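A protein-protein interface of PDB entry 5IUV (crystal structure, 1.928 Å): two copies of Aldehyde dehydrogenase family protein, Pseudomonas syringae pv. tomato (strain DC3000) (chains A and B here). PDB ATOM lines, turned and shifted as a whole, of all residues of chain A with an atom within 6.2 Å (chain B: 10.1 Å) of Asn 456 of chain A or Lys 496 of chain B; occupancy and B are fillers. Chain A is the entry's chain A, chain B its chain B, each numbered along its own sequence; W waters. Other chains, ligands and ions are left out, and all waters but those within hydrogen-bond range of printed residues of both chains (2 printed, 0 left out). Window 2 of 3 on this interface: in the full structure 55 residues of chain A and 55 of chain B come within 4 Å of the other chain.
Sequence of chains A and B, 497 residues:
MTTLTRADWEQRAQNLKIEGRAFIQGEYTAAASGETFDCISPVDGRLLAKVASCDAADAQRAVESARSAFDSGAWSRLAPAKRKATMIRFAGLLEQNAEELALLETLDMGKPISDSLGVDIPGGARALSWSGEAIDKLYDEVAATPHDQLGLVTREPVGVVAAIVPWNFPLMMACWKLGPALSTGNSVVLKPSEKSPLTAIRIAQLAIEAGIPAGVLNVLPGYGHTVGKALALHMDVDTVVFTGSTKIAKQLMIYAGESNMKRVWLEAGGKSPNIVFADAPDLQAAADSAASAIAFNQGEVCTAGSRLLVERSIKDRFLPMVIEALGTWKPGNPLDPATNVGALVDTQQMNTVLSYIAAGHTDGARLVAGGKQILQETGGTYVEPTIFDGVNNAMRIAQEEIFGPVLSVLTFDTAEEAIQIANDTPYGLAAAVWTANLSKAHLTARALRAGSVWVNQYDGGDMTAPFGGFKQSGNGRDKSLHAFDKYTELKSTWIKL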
ATOM      1  N   ALA A 280     -15.887 -17.925  -1.195  1.00  0.00           N
ATOM      2  CA  ALA A 280     -16.408 -19.242  -1.561  1.00  0.00           C
ATOM      3  C   ALA A 280     -15.416 -19.943  -2.483  1.00  0.00           C
ATOM      4  O   ALA A 280     -14.849 -19.311  -3.372  1.00  0.00           O
ATOM      5  CB  ALA A 280     -17.775 -19.119  -2.246  1.00  0.00           C
ATOM      6  N   PRO A 281     -15.195 -21.251  -2.272  1.00  0.00           N
ATOM      7  CA  PRO A 281     -14.183 -21.969  -3.062  1.00  0.00           C
ATOM      8  C   PRO A 281     -14.528 -22.056  -4.551  1.00  0.00           C
ATOM      9  O   PRO A 281     -13.631 -22.054  -5.391  1.00  0.00           O
ATOM     10  CB  PRO A 281     -14.158 -23.368  -2.426  1.00  0.00           C
ATOM     11  CG  PRO A 281     -15.440 -23.493  -1.692  1.00  0.00           C
ATOM     12  CD  PRO A 281     -15.805 -22.106  -1.238  1.00  0.00           C
ATOM     13  N   ALA A 432     -27.427 -22.196   4.637  1.00  0.00           N
ATOM     14  CA  ALA A 432     -26.167 -22.632   4.034  1.00  0.00           C
ATOM     15  C   ALA A 432     -25.095 -21.548   4.073  1.00  0.00           C
ATOM     16  O   ALA A 432     -25.396 -20.351   4.092  1.00  0.00           O
ATOM     17  CB  ALA A 432     -26.388 -23.091   2.602  1.00  0.00           C
ATOM     18  N   VAL A 433     -23.839 -21.987   4.089  1.00  0.00           N
ATOM     19  CA  VAL A 433     -22.691 -21.088   4.155  1.00  0.00           C
ATOM     20  C   VAL A 433     -21.662 -21.491   3.118  1.00  0.00           C
ATOM     21  O   VAL A 433     -21.299 -22.659   3.036  1.00  0.00           O
ATOM     22  CB  VAL A 433     -22.017 -21.109   5.543  1.00  0.00           C
ATOM     23  CG1 VAL A 433     -20.887 -20.092   5.591  1.00  0.00           C
ATOM     24  CG2 VAL A 433     -23.026 -20.827   6.625  1.00  0.00           C
ATOM     25  N   TRP A 434     -21.187 -20.528   2.336  1.00  0.00           N
ATOM     26  CA  TRP A 434     -20.179 -20.810   1.326  1.00  0.00           C
ATOM     27  C   TRP A 434     -18.925 -20.005   1.622  1.00  0.00           C
ATOM     28  O   TRP A 434     -18.921 -18.779   1.495  1.00  0.00           O
ATOM     29  CB  TRP A 434     -20.703 -20.491  -0.082  1.00  0.00           C
ATOM     30  CG  TRP A 434     -21.944 -21.260  -0.468  1.00  0.00           C
ATOM     31  CD1 TRP A 434     -23.216 -21.044  -0.020  1.00  0.00           C
ATOM     32  CD2 TRP A 434     -22.028 -22.356  -1.394  1.00  0.00           C
ATOM     33  NE1 TRP A 434     -24.083 -21.942  -0.600  1.00  0.00           N
ATOM     34  CE2 TRP A 434     -23.378 -22.754  -1.450  1.00  0.00           C
ATOM     35  CE3 TRP A 434     -21.090 -23.036  -2.180  1.00  0.00           C
ATOM     36  CZ2 TRP A 434     -23.816 -23.803  -2.262  1.00  0.00           C
ATOM     37  CZ3 TRP A 434     -21.526 -24.076  -2.988  1.00  0.00           C
ATOM     38  CH2 TRP A 434     -22.879 -24.447  -3.023  1.00  0.00           C
ATOM     39  N   THR A 435     -17.867 -20.703   2.030  1.00  0.00           N
ATOM     40  CA  THR A 435     -16.582 -20.071   2.326  1.00  0.00           C
ATOM     41  C   THR A 435     -15.473 -21.115   2.367  1.00  0.00           C
ATOM     42  O   THR A 435     -15.698 -22.247   2.780  1.00  0.00           O
ATOM     43  CB  THR A 435     -16.600 -19.301   3.672  1.00  0.00           C
ATOM     44  OG1 THR A 435     -15.276 -18.854   3.981  1.00  0.00           O
ATOM     45  CG2 THR A 435     -17.088 -20.188   4.803  1.00  0.00           C
ATOM     46  N   ALA A 436     -14.277 -20.727   1.941  1.00  0.00           N
ATOM     47  CA  ALA A 436     -13.134 -21.634   1.952  1.00  0.00           C
ATOM     48  C   ALA A 436     -12.362 -21.550   3.264  1.00  0.00           C
ATOM     49  O   ALA A 436     -11.428 -22.313   3.491  1.00  0.00           O
ATOM     50  CB  ALA A 436     -12.204 -21.333   0.774  1.00  0.00           C
ATOM     51  N   ALA A 441     -16.096 -20.868   8.346  1.00  0.00           N
ATOM     52  CA  ALA A 441     -17.083 -21.900   8.048  1.00  0.00           C
ATOM     53  C   ALA A 441     -17.713 -22.461   9.325  1.00  0.00           C
ATOM     54  O   ALA A 441     -18.939 -22.532   9.442  1.00  0.00           O
ATOM     55  CB  ALA A 441     -16.459 -23.022   7.227  1.00  0.00           C
ATOM     56  N   TRP A 454     -25.746 -26.280   5.773  1.00  0.00           N
ATOM     57  CA  TRP A 454     -24.975 -26.870   4.693  1.00  0.00           C
ATOM     58  C   TRP A 454     -23.803 -25.964   4.338  1.00  0.00           C
ATOM     59  O   TRP A 454     -23.967 -24.760   4.153  1.00  0.00           O
ATOM     60  CB  TRP A 454     -25.880 -27.139   3.481  1.00  0.00           C
ATOM     61  CG  TRP A 454     -26.990 -28.101   3.822  1.00  0.00           C
ATOM     62  CD1 TRP A 454     -26.849 -29.321   4.418  1.00  0.00           C
ATOM     63  CD2 TRP A 454     -28.399 -27.920   3.616  1.00  0.00           C
ATOM     64  NE1 TRP A 454     -28.079 -29.913   4.590  1.00  0.00           N
ATOM     65  CE2 TRP A 454     -29.046 -29.075   4.103  1.00  0.00           C
ATOM     66  CE3 TRP A 454     -29.177 -26.898   3.058  1.00  0.00           C
ATOM     67  CZ2 TRP A 454     -30.431 -29.238   4.058  1.00  0.00           C
ATOM     68  CZ3 TRP A 454     -30.561 -27.063   3.011  1.00  0.00           C
ATOM     69  CH2 TRP A 454     -31.169 -28.225   3.502  1.00  0.00           C
ATOM     70  N   VAL A 455     -22.610 -26.538   4.273  1.00  0.00           N
ATOM     71  CA  VAL A 455     -21.415 -25.738   4.026  1.00  0.00           C
ATOM     72  C   VAL A 455     -20.800 -26.118   2.690  1.00  0.00           C
ATOM     73  O   VAL A 455     -20.488 -27.287   2.449  1.00  0.00           O
ATOM     74  CB  VAL A 455     -20.365 -25.903   5.148  1.00  0.00           C
ATOM     75  CG1 VAL A 455     -19.115 -25.054   4.853  1.00  0.00           C
ATOM     76  CG2 VAL A 455     -20.970 -25.529   6.496  1.00  0.00           C
ATOM     77  N   ASN A 456     -20.656 -25.118   1.827  1.00  0.00           N
ATOM     78  CA  ASN A 456     -20.129 -25.279   0.471  1.00  0.00           C
ATOM     79  C   ASN A 456     -20.926 -26.279  -0.359  1.00  0.00           C
ATOM     80  O   ASN A 456     -20.397 -26.952  -1.242  1.00  0.00           O
ATOM     81  CB  ASN A 456     -18.651 -25.649   0.532  1.00  0.00           C
ATOM     82  CG  ASN A 456     -17.821 -24.527   1.104  1.00  0.00           C
ATOM     83  OD1 ASN A 456     -18.230 -23.367   1.040  1.00  0.00           O
ATOM     84  ND2 ASN A 456     -16.672 -24.852   1.679  1.00  0.00           N
ATOM     85  N   GLN A 457     -22.219 -26.332  -0.066  1.00  0.00           N
ATOM     86  CA  GLN A 457     -23.180 -27.108  -0.825  1.00  0.00           C
ATOM     87  C   GLN A 457     -24.570 -26.655  -0.396  1.00  0.00           C
ATOM     88  O   GLN A 457     -24.704 -25.940   0.600  1.00  0.00           O
ATOM     89  CB  GLN A 457     -23.000 -28.607  -0.580  1.00  0.00           C
ATOM     90  CG  GLN A 457     -23.360 -29.033   0.830  1.00  0.00           C
ATOM     91  CD  GLN A 457     -23.007 -30.482   1.097  1.00  0.00           C
ATOM     92  OE1 GLN A 457     -23.081 -31.319   0.205  1.00  0.00           O
ATOM     93  NE2 GLN A 457     -22.610 -30.780   2.330  1.00  0.00           N
ATOM     94  N   TYR A 458     -25.596 -27.053  -1.139  1.00  0.00           N
ATOM     95  CA  TYR A 458     -26.969 -26.851  -0.678  1.00  0.00           C
ATOM     96  C   TYR A 458     -27.730 -28.169  -0.735  1.00  0.00           C
ATOM     97  O   TYR A 458     -27.387 -29.042  -1.523  1.00  0.00           O
ATOM     98  CB  TYR A 458     -27.699 -25.774  -1.501  1.00  0.00           C
ATOM     99  CG  TYR A 458     -28.820 -25.156  -0.703  1.00  0.00           C
ATOM    100  CD1 TYR A 458     -28.568 -24.114   0.166  1.00  0.00           C
ATOM    101  CD2 TYR A 458     -30.117 -25.652  -0.776  1.00  0.00           C
ATOM    102  CE1 TYR A 458     -29.569 -23.561   0.931  1.00  0.00           C
ATOM    103  CE2 TYR A 458     -31.137 -25.105  -0.011  1.00  0.00           C
ATOM    104  CZ  TYR A 458     -30.850 -24.056   0.843  1.00  0.00           C
ATOM    105  OH  TYR A 458     -31.837 -23.491   1.625  1.00  0.00           O
ATOM    106  N   THR B 145     -20.306 -40.788   6.340  1.00  0.00           N
ATOM    107  CA  THR B 145     -20.589 -40.061   5.104  1.00  0.00           C
ATOM    108  C   THR B 145     -19.563 -40.408   4.031  1.00  0.00           C
ATOM    109  O   THR B 145     -18.529 -41.005   4.337  1.00  0.00           O
ATOM    110  CB  THR B 145     -20.568 -38.531   5.343  1.00  0.00           C
ATOM    111  OG1 THR B 145     -19.269 -38.147   5.813  1.00  0.00           O
ATOM    112  CG2 THR B 145     -21.606 -38.129   6.371  1.00  0.00           C
ATOM    113  N   PRO B 146     -19.833 -40.035   2.769  1.00  0.00           N
ATOM    114  CA  PRO B 146     -18.790 -40.188   1.751  1.00  0.00           C
ATOM    115  C   PRO B 146     -17.532 -39.390   2.090  1.00  0.00           C
ATOM    116  O   PRO B 146     -17.560 -38.524   2.970  1.00  0.00           O
ATOM    117  CB  PRO B 146     -19.456 -39.648   0.483  1.00  0.00           C
ATOM    118  CG  PRO B 146     -20.890 -39.911   0.695  1.00  0.00           C
ATOM    119  CD  PRO B 146     -21.130 -39.684   2.165  1.00  0.00           C
ATOM    120  N   HIS B 147     -16.447 -39.686   1.385  1.00  0.00           N
ATOM    121  CA  HIS B 147     -15.135 -39.124   1.688  1.00  0.00           C
ATOM    122  C   HIS B 147     -15.061 -37.597   1.550  1.00  0.00           C
ATOM    123  O   HIS B 147     -14.213 -36.957   2.174  1.00  0.00           O
ATOM    124  CB  HIS B 147     -14.079 -39.760   0.775  1.00  0.00           C
ATOM    125  CG  HIS B 147     -14.034 -39.166  -0.595  1.00  0.00           C
ATOM    126  ND1 HIS B 147     -14.881 -39.565  -1.618  1.00  0.00           N
ATOM    127  CD2 HIS B 147     -13.259 -38.189  -1.126  1.00  0.00           C
ATOM    128  CE1 HIS B 147     -14.625 -38.867  -2.701  1.00  0.00           C
ATOM    129  NE2 HIS B 147     -13.641 -38.019  -2.432  1.00  0.00           N
ATOM    130  N   ASP B 148     -15.935 -37.017   0.730  1.00  0.00           N
ATOM    131  CA  ASP B 148     -15.904 -35.575   0.496  1.00  0.00           C
ATOM    132  C   ASP B 148     -16.926 -34.824   1.355  1.00  0.00           C
ATOM    133  O   ASP B 148     -17.259 -33.669   1.085  1.00  0.00           O
ATOM    134  CB  ASP B 148     -16.139 -35.276  -0.991  1.00  0.00           C
ATOM    135  CG  ASP B 148     -17.507 -35.727  -1.472  1.00  0.00           C
ATOM    136  OD1 ASP B 148     -18.141 -36.560  -0.794  1.00  0.00           O
ATOM    137  OD2 ASP B 148     -17.954 -35.250  -2.534  1.00  0.00           O
ATOM    138  N   GLN B 149     -17.416 -35.489   2.395  1.00  0.00           N
ATOM    139  CA  GLN B 149     -18.395 -34.893   3.292  1.00  0.00           C
ATOM    140  C   GLN B 149     -17.966 -35.066   4.731  1.00  0.00           C
ATOM    141  O   GLN B 149     -17.462 -36.122   5.110  1.00  0.00           O
ATOM    142  CB  GLN B 149     -19.778 -35.529   3.102  1.00  0.00           C
ATOM    143  CG  GLN B 149     -20.386 -35.364   1.723  1.00  0.00           C
ATOM    144  CD  GLN B 149     -21.042 -34.014   1.533  1.00  0.00           C
ATOM    145  OE1 GLN B 149     -21.538 -33.407   2.484  1.00  0.00           O
ATOM    146  NE2 GLN B 149     -21.046 -33.532   0.301  1.00  0.00           N
ATOM    147  N   LEU B 150     -18.177 -34.033   5.537  1.00  0.00           N
ATOM    148  CA  LEU B 150     -18.095 -34.173   6.985  1.00  0.00           C
ATOM    149  C   LEU B 150     -19.459 -33.849   7.578  1.00  0.00           C
ATOM    150  O   LEU B 150     -19.950 -32.722   7.449  1.00  0.00           O
ATOM    151  CB  LEU B 150     -17.009 -33.268   7.575  1.00  0.00           C
ATOM    152  CG  LEU B 150     -16.984 -33.191   9.107  1.00  0.00           C
ATOM    153  CD1 LEU B 150     -16.740 -34.560   9.719  1.00  0.00           C
ATOM    154  CD2 LEU B 150     -15.928 -32.204   9.593  1.00  0.00           C
ATOM    155  N   GLY B 151     -20.079 -34.843   8.209  1.00  0.00           N
ATOM    156  CA  GLY B 151     -21.424 -34.677   8.739  1.00  0.00           C
ATOM    157  C   GLY B 151     -21.448 -34.618  10.259  1.00  0.00           C
ATOM    158  O   GLY B 151     -21.273 -35.632  10.930  1.00  0.00           O
ATOM    159  N   LEU B 152     -21.665 -33.425  10.798  1.00  0.00           N
ATOM    160  CA  LEU B 152     -21.720 -33.230  12.243  1.00  0.00           C
ATOM    161  C   LEU B 152     -23.159 -33.142  12.725  1.00  0.00           C
ATOM    162  O   LEU B 152     -23.976 -32.456  12.119  1.00  0.00           O
ATOM    163  CB  LEU B 152     -20.966 -31.963  12.652  1.00  0.00           C
ATOM    164  CG  LEU B 152     -19.533 -31.807  12.154  1.00  0.00           C
ATOM    165  CD1 LEU B 152     -18.981 -30.459  12.591  1.00  0.00           C
ATOM    166  CD2 LEU B 152     -18.665 -32.951  12.675  1.00  0.00           C
ATOM    167  N   THR B 493     -24.812 -30.334  10.602  1.00  0.00           N
ATOM    168  CA  THR B 493     -23.920 -29.516   9.790  1.00  0.00           C
ATOM    169  C   THR B 493     -23.214 -30.417   8.782  1.00  0.00           C
ATOM    170  O   THR B 493     -22.354 -31.214   9.156  1.00  0.00           O
ATOM    171  CB  THR B 493     -22.878 -28.763  10.656  1.00  0.00           C
ATOM    172  OG1 THR B 493     -23.551 -27.977  11.653  1.00  0.00           O
ATOM    173  CG2 THR B 493     -22.024 -27.841   9.793  1.00  0.00           C
ATOM    174  N   TRP B 494     -23.600 -30.311   7.514  1.00  0.00           N
ATOM    175  CA  TRP B 494     -23.027 -31.157   6.470  1.00  0.00           C
ATOM    176  C   TRP B 494     -22.084 -30.340   5.602  1.00  0.00           C
ATOM    177  O   TRP B 494     -22.500 -29.430   4.881  1.00  0.00           O
ATOM    178  CB  TRP B 494     -24.130 -31.813   5.624  1.00  0.00           C
ATOM    179  CG  TRP B 494     -24.203 -33.317   5.819  1.00  0.00           C
ATOM    180  CD1 TRP B 494     -23.932 -34.282   4.890  1.00  0.00           C
ATOM    181  CD2 TRP B 494     -24.550 -34.009   7.026  1.00  0.00           C
ATOM    182  NE1 TRP B 494     -24.096 -35.530   5.444  1.00  0.00           N
ATOM    183  CE2 TRP B 494     -24.481 -35.391   6.752  1.00  0.00           C
ATOM    184  CE3 TRP B 494     -24.918 -33.594   8.310  1.00  0.00           C
ATOM    185  CZ2 TRP B 494     -24.762 -36.362   7.719  1.00  0.00           C
ATOM    186  CZ3 TRP B 494     -25.189 -34.560   9.273  1.00  0.00           C
ATOM    187  CH2 TRP B 494     -25.109 -35.925   8.971  1.00  0.00           C
ATOM    188  N   ILE B 495     -20.804 -30.681   5.689  1.00  0.00           N
ATOM    189  CA  ILE B 495     -19.744 -29.892   5.076  1.00  0.00           C
ATOM    190  C   ILE B 495     -19.139 -30.596   3.874  1.00  0.00           C
ATOM    191  O   ILE B 495     -18.620 -31.708   3.992  1.00  0.00           O
ATOM    192  CB  ILE B 495     -18.624 -29.590   6.101  1.00  0.00           C
ATOM    193  CG1 ILE B 495     -19.215 -28.922   7.349  1.00  0.00           C
ATOM    194  CG2 ILE B 495     -17.540 -28.736   5.465  1.00  0.00           C
ATOM    195  CD1 ILE B 495     -18.301 -28.975   8.573  1.00  0.00           C
ATOM    196  N   LYS B 496     -19.200 -29.947   2.717  1.00  0.00           N
ATOM    197  CA  LYS B 496     -18.581 -30.482   1.517  1.00  0.00           C
ATOM    198  C   LYS B 496     -17.109 -30.088   1.499  1.00  0.00           C
ATOM    199  O   LYS B 496     -16.774 -28.906   1.636  1.00  0.00           O
ATOM    200  CB  LYS B 496     -19.288 -29.975   0.260  1.00  0.00           C
ATOM    201  CG  LYS B 496     -18.608 -30.390  -1.036  1.00  0.00           C
ATOM    202  CD  LYS B 496     -19.464 -31.362  -1.823  1.00  0.00           C
ATOM    203  CE  LYS B 496     -18.916 -31.569  -3.231  1.00  0.00           C
ATOM    204  NZ  LYS B 496     -17.496 -32.013  -3.179  1.00  0.00           N
ATOM    205  N   LEU B 497     -16.240 -31.083   1.336  1.00  0.00           N
ATOM    206  CA  LEU B 497     -14.790 -30.889   1.450  1.00  0.00           C
ATOM    207  C   LEU B 497     -14.105 -30.871   0.088  1.00  0.00           C
ATOM    208  O   LEU B 497     -14.517 -31.597  -0.811  1.00  0.00           O
ATOM    209  CB  LEU B 497     -14.182 -31.990   2.320  1.00  0.00           C
ATOM    210  CG  LEU B 497     -14.732 -32.024   3.746  1.00  0.00           C
ATOM    211  CD1 LEU B 497     -14.250 -33.261   4.508  1.00  0.00           C
ATOM    212  CD2 LEU B 497     -14.360 -30.735   4.485  1.00  0.00           C
HETATM  213  O   HOH W   1     -24.449 -33.926   1.284  1.00  0.00           O
HETATM  214  O   HOH W   2     -14.993 -27.209   0.768  1.00  0.00           O
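Of the 13 printed residues of chain B, 4 touch a printed residue of chain A.
Printed residues of chain A that touch a printed residue of chain B: Trp 454, Val 455, Asn 456 and Gln 457.
Hydrophobic or aromatic side chains of chain A that line the printed part of chain B: Trp 454 and Val 455.
Of chain B, only Lys 496 comes within 4 Å of Asn 456 of chain A.
Printed residues of chain A within 4 Å of Lys 496 of chain B: Val 455 (3.0 Å), Asn 456 (3.6 Å) and Gln 457 (3.5 Å).
Val 455 of chain A touches just these residues of chain B: Trp 494 (3.0 Å), Ile 495 (3.8 Å) and Lys 496 (3.0 Å).
Gln 457 of chain A touches just these residues of chain B: Gln 149 (2.8 Å), Trp 494 (2.9 Å), Ile 495 (3.8 Å) and Lys 496 (3.5 Å).
Printed residues of chain A within 4 Å of Trp 494 of chain B: Trp 454, Val 455 and Gln 457.
Of the printed residues of chain A, Ile 495 of chain B touches Val 455 and Gln 457.
Of the printed residues of chain A, Gln 149 of chain B touches Gln 457.
Printed residues of chain B within 4 Å of Trp 454 of chain A: Trp 494 (3.6 Å).
Ala 280 of chain A touches none of the printed residues of chain B.
The nearest printed residue of chain A that does not touch Lys 496 of chain B is Trp 454 of chain A (6.3 Å).
The nearest printed residue of chain A that does not touch Trp 494 of chain B is Asn 456 of chain A (5.6 Å).
Water W2 bridges the backbone carbonyl oxygen (O) of Lys 496 of chain B (2.6 Å) and the side-chain amide nitrogen (ND2) of Asn 456 of chain A (3.0 Å).
Water W1 lies within hydrogen-bond range of the side-chain amide oxygen of Gln 457 of chain A (3.1 Å) and the side-chain amide oxygen of Gln 149 of chain B (3.2 Å).
Trp 494 of chain B touches Trp 454 of chain A.
Val 455 of chain A touches Ile 495 of chain B (O to CA, 3.8 Å).
Asn 456 of chain A touches Lys 496 of chain B (O to CB, 3.6 Å).
Gln 457 of chain A touches Ile 495 of chain B.
Lys 496 of chain B touches Gln 457 of chain A (N to NE2, 3.5 Å).
No position is printed for both chains.
The backbone NH (N) of Val 455 of chain A lies within hydrogen-bond range of the backbone carbonyl oxygen (O) of Trp 494 of chain B, at 3.0 Å.
The backbone carbonyl oxygen of Val 455 of chain A lies within hydrogen-bond range of the backbone NH of Lys 496 of chain B (3.0 Å).
The side-chain amide nitrogen of Gln 457 of chain A lies within hydrogen-bond range of the side-chain amide oxygen of Gln 149 of chain B (2.8 Å).
NE2 of Gln 457 of chain A is in hydrogen-bond range of O of Trp 494 of chain B, at 2.9 Å.
O of Trp 454 of chain A sits at hydrogen-bond distance from N of Val 433 of chain A, at 2.8 Å.
The backbone carbonyl oxygen (O) of Val 433 of chain A is in hydrogen-bond range of the backbone NH (N) of Asn 456 of chain A (2.8 Å).
The backbone NH of Thr 435 of chain A is in hydrogen-bond range of the side-chain amide oxygen of Asn 456 of chain A (2.9 Å).
OG1 of Thr 145 of chain B lies within hydrogen-bond range of O of Gln 149 of chain B, at 2.8 Å.
NZ of Lys 496 of chain B is in salt-bridge range of OD2 of Asp 148 of chain B (3.3 Å).
N of Leu 150 of chain B lies within hydrogen-bond range of O of Ile 495 of chain B (2.8 Å).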
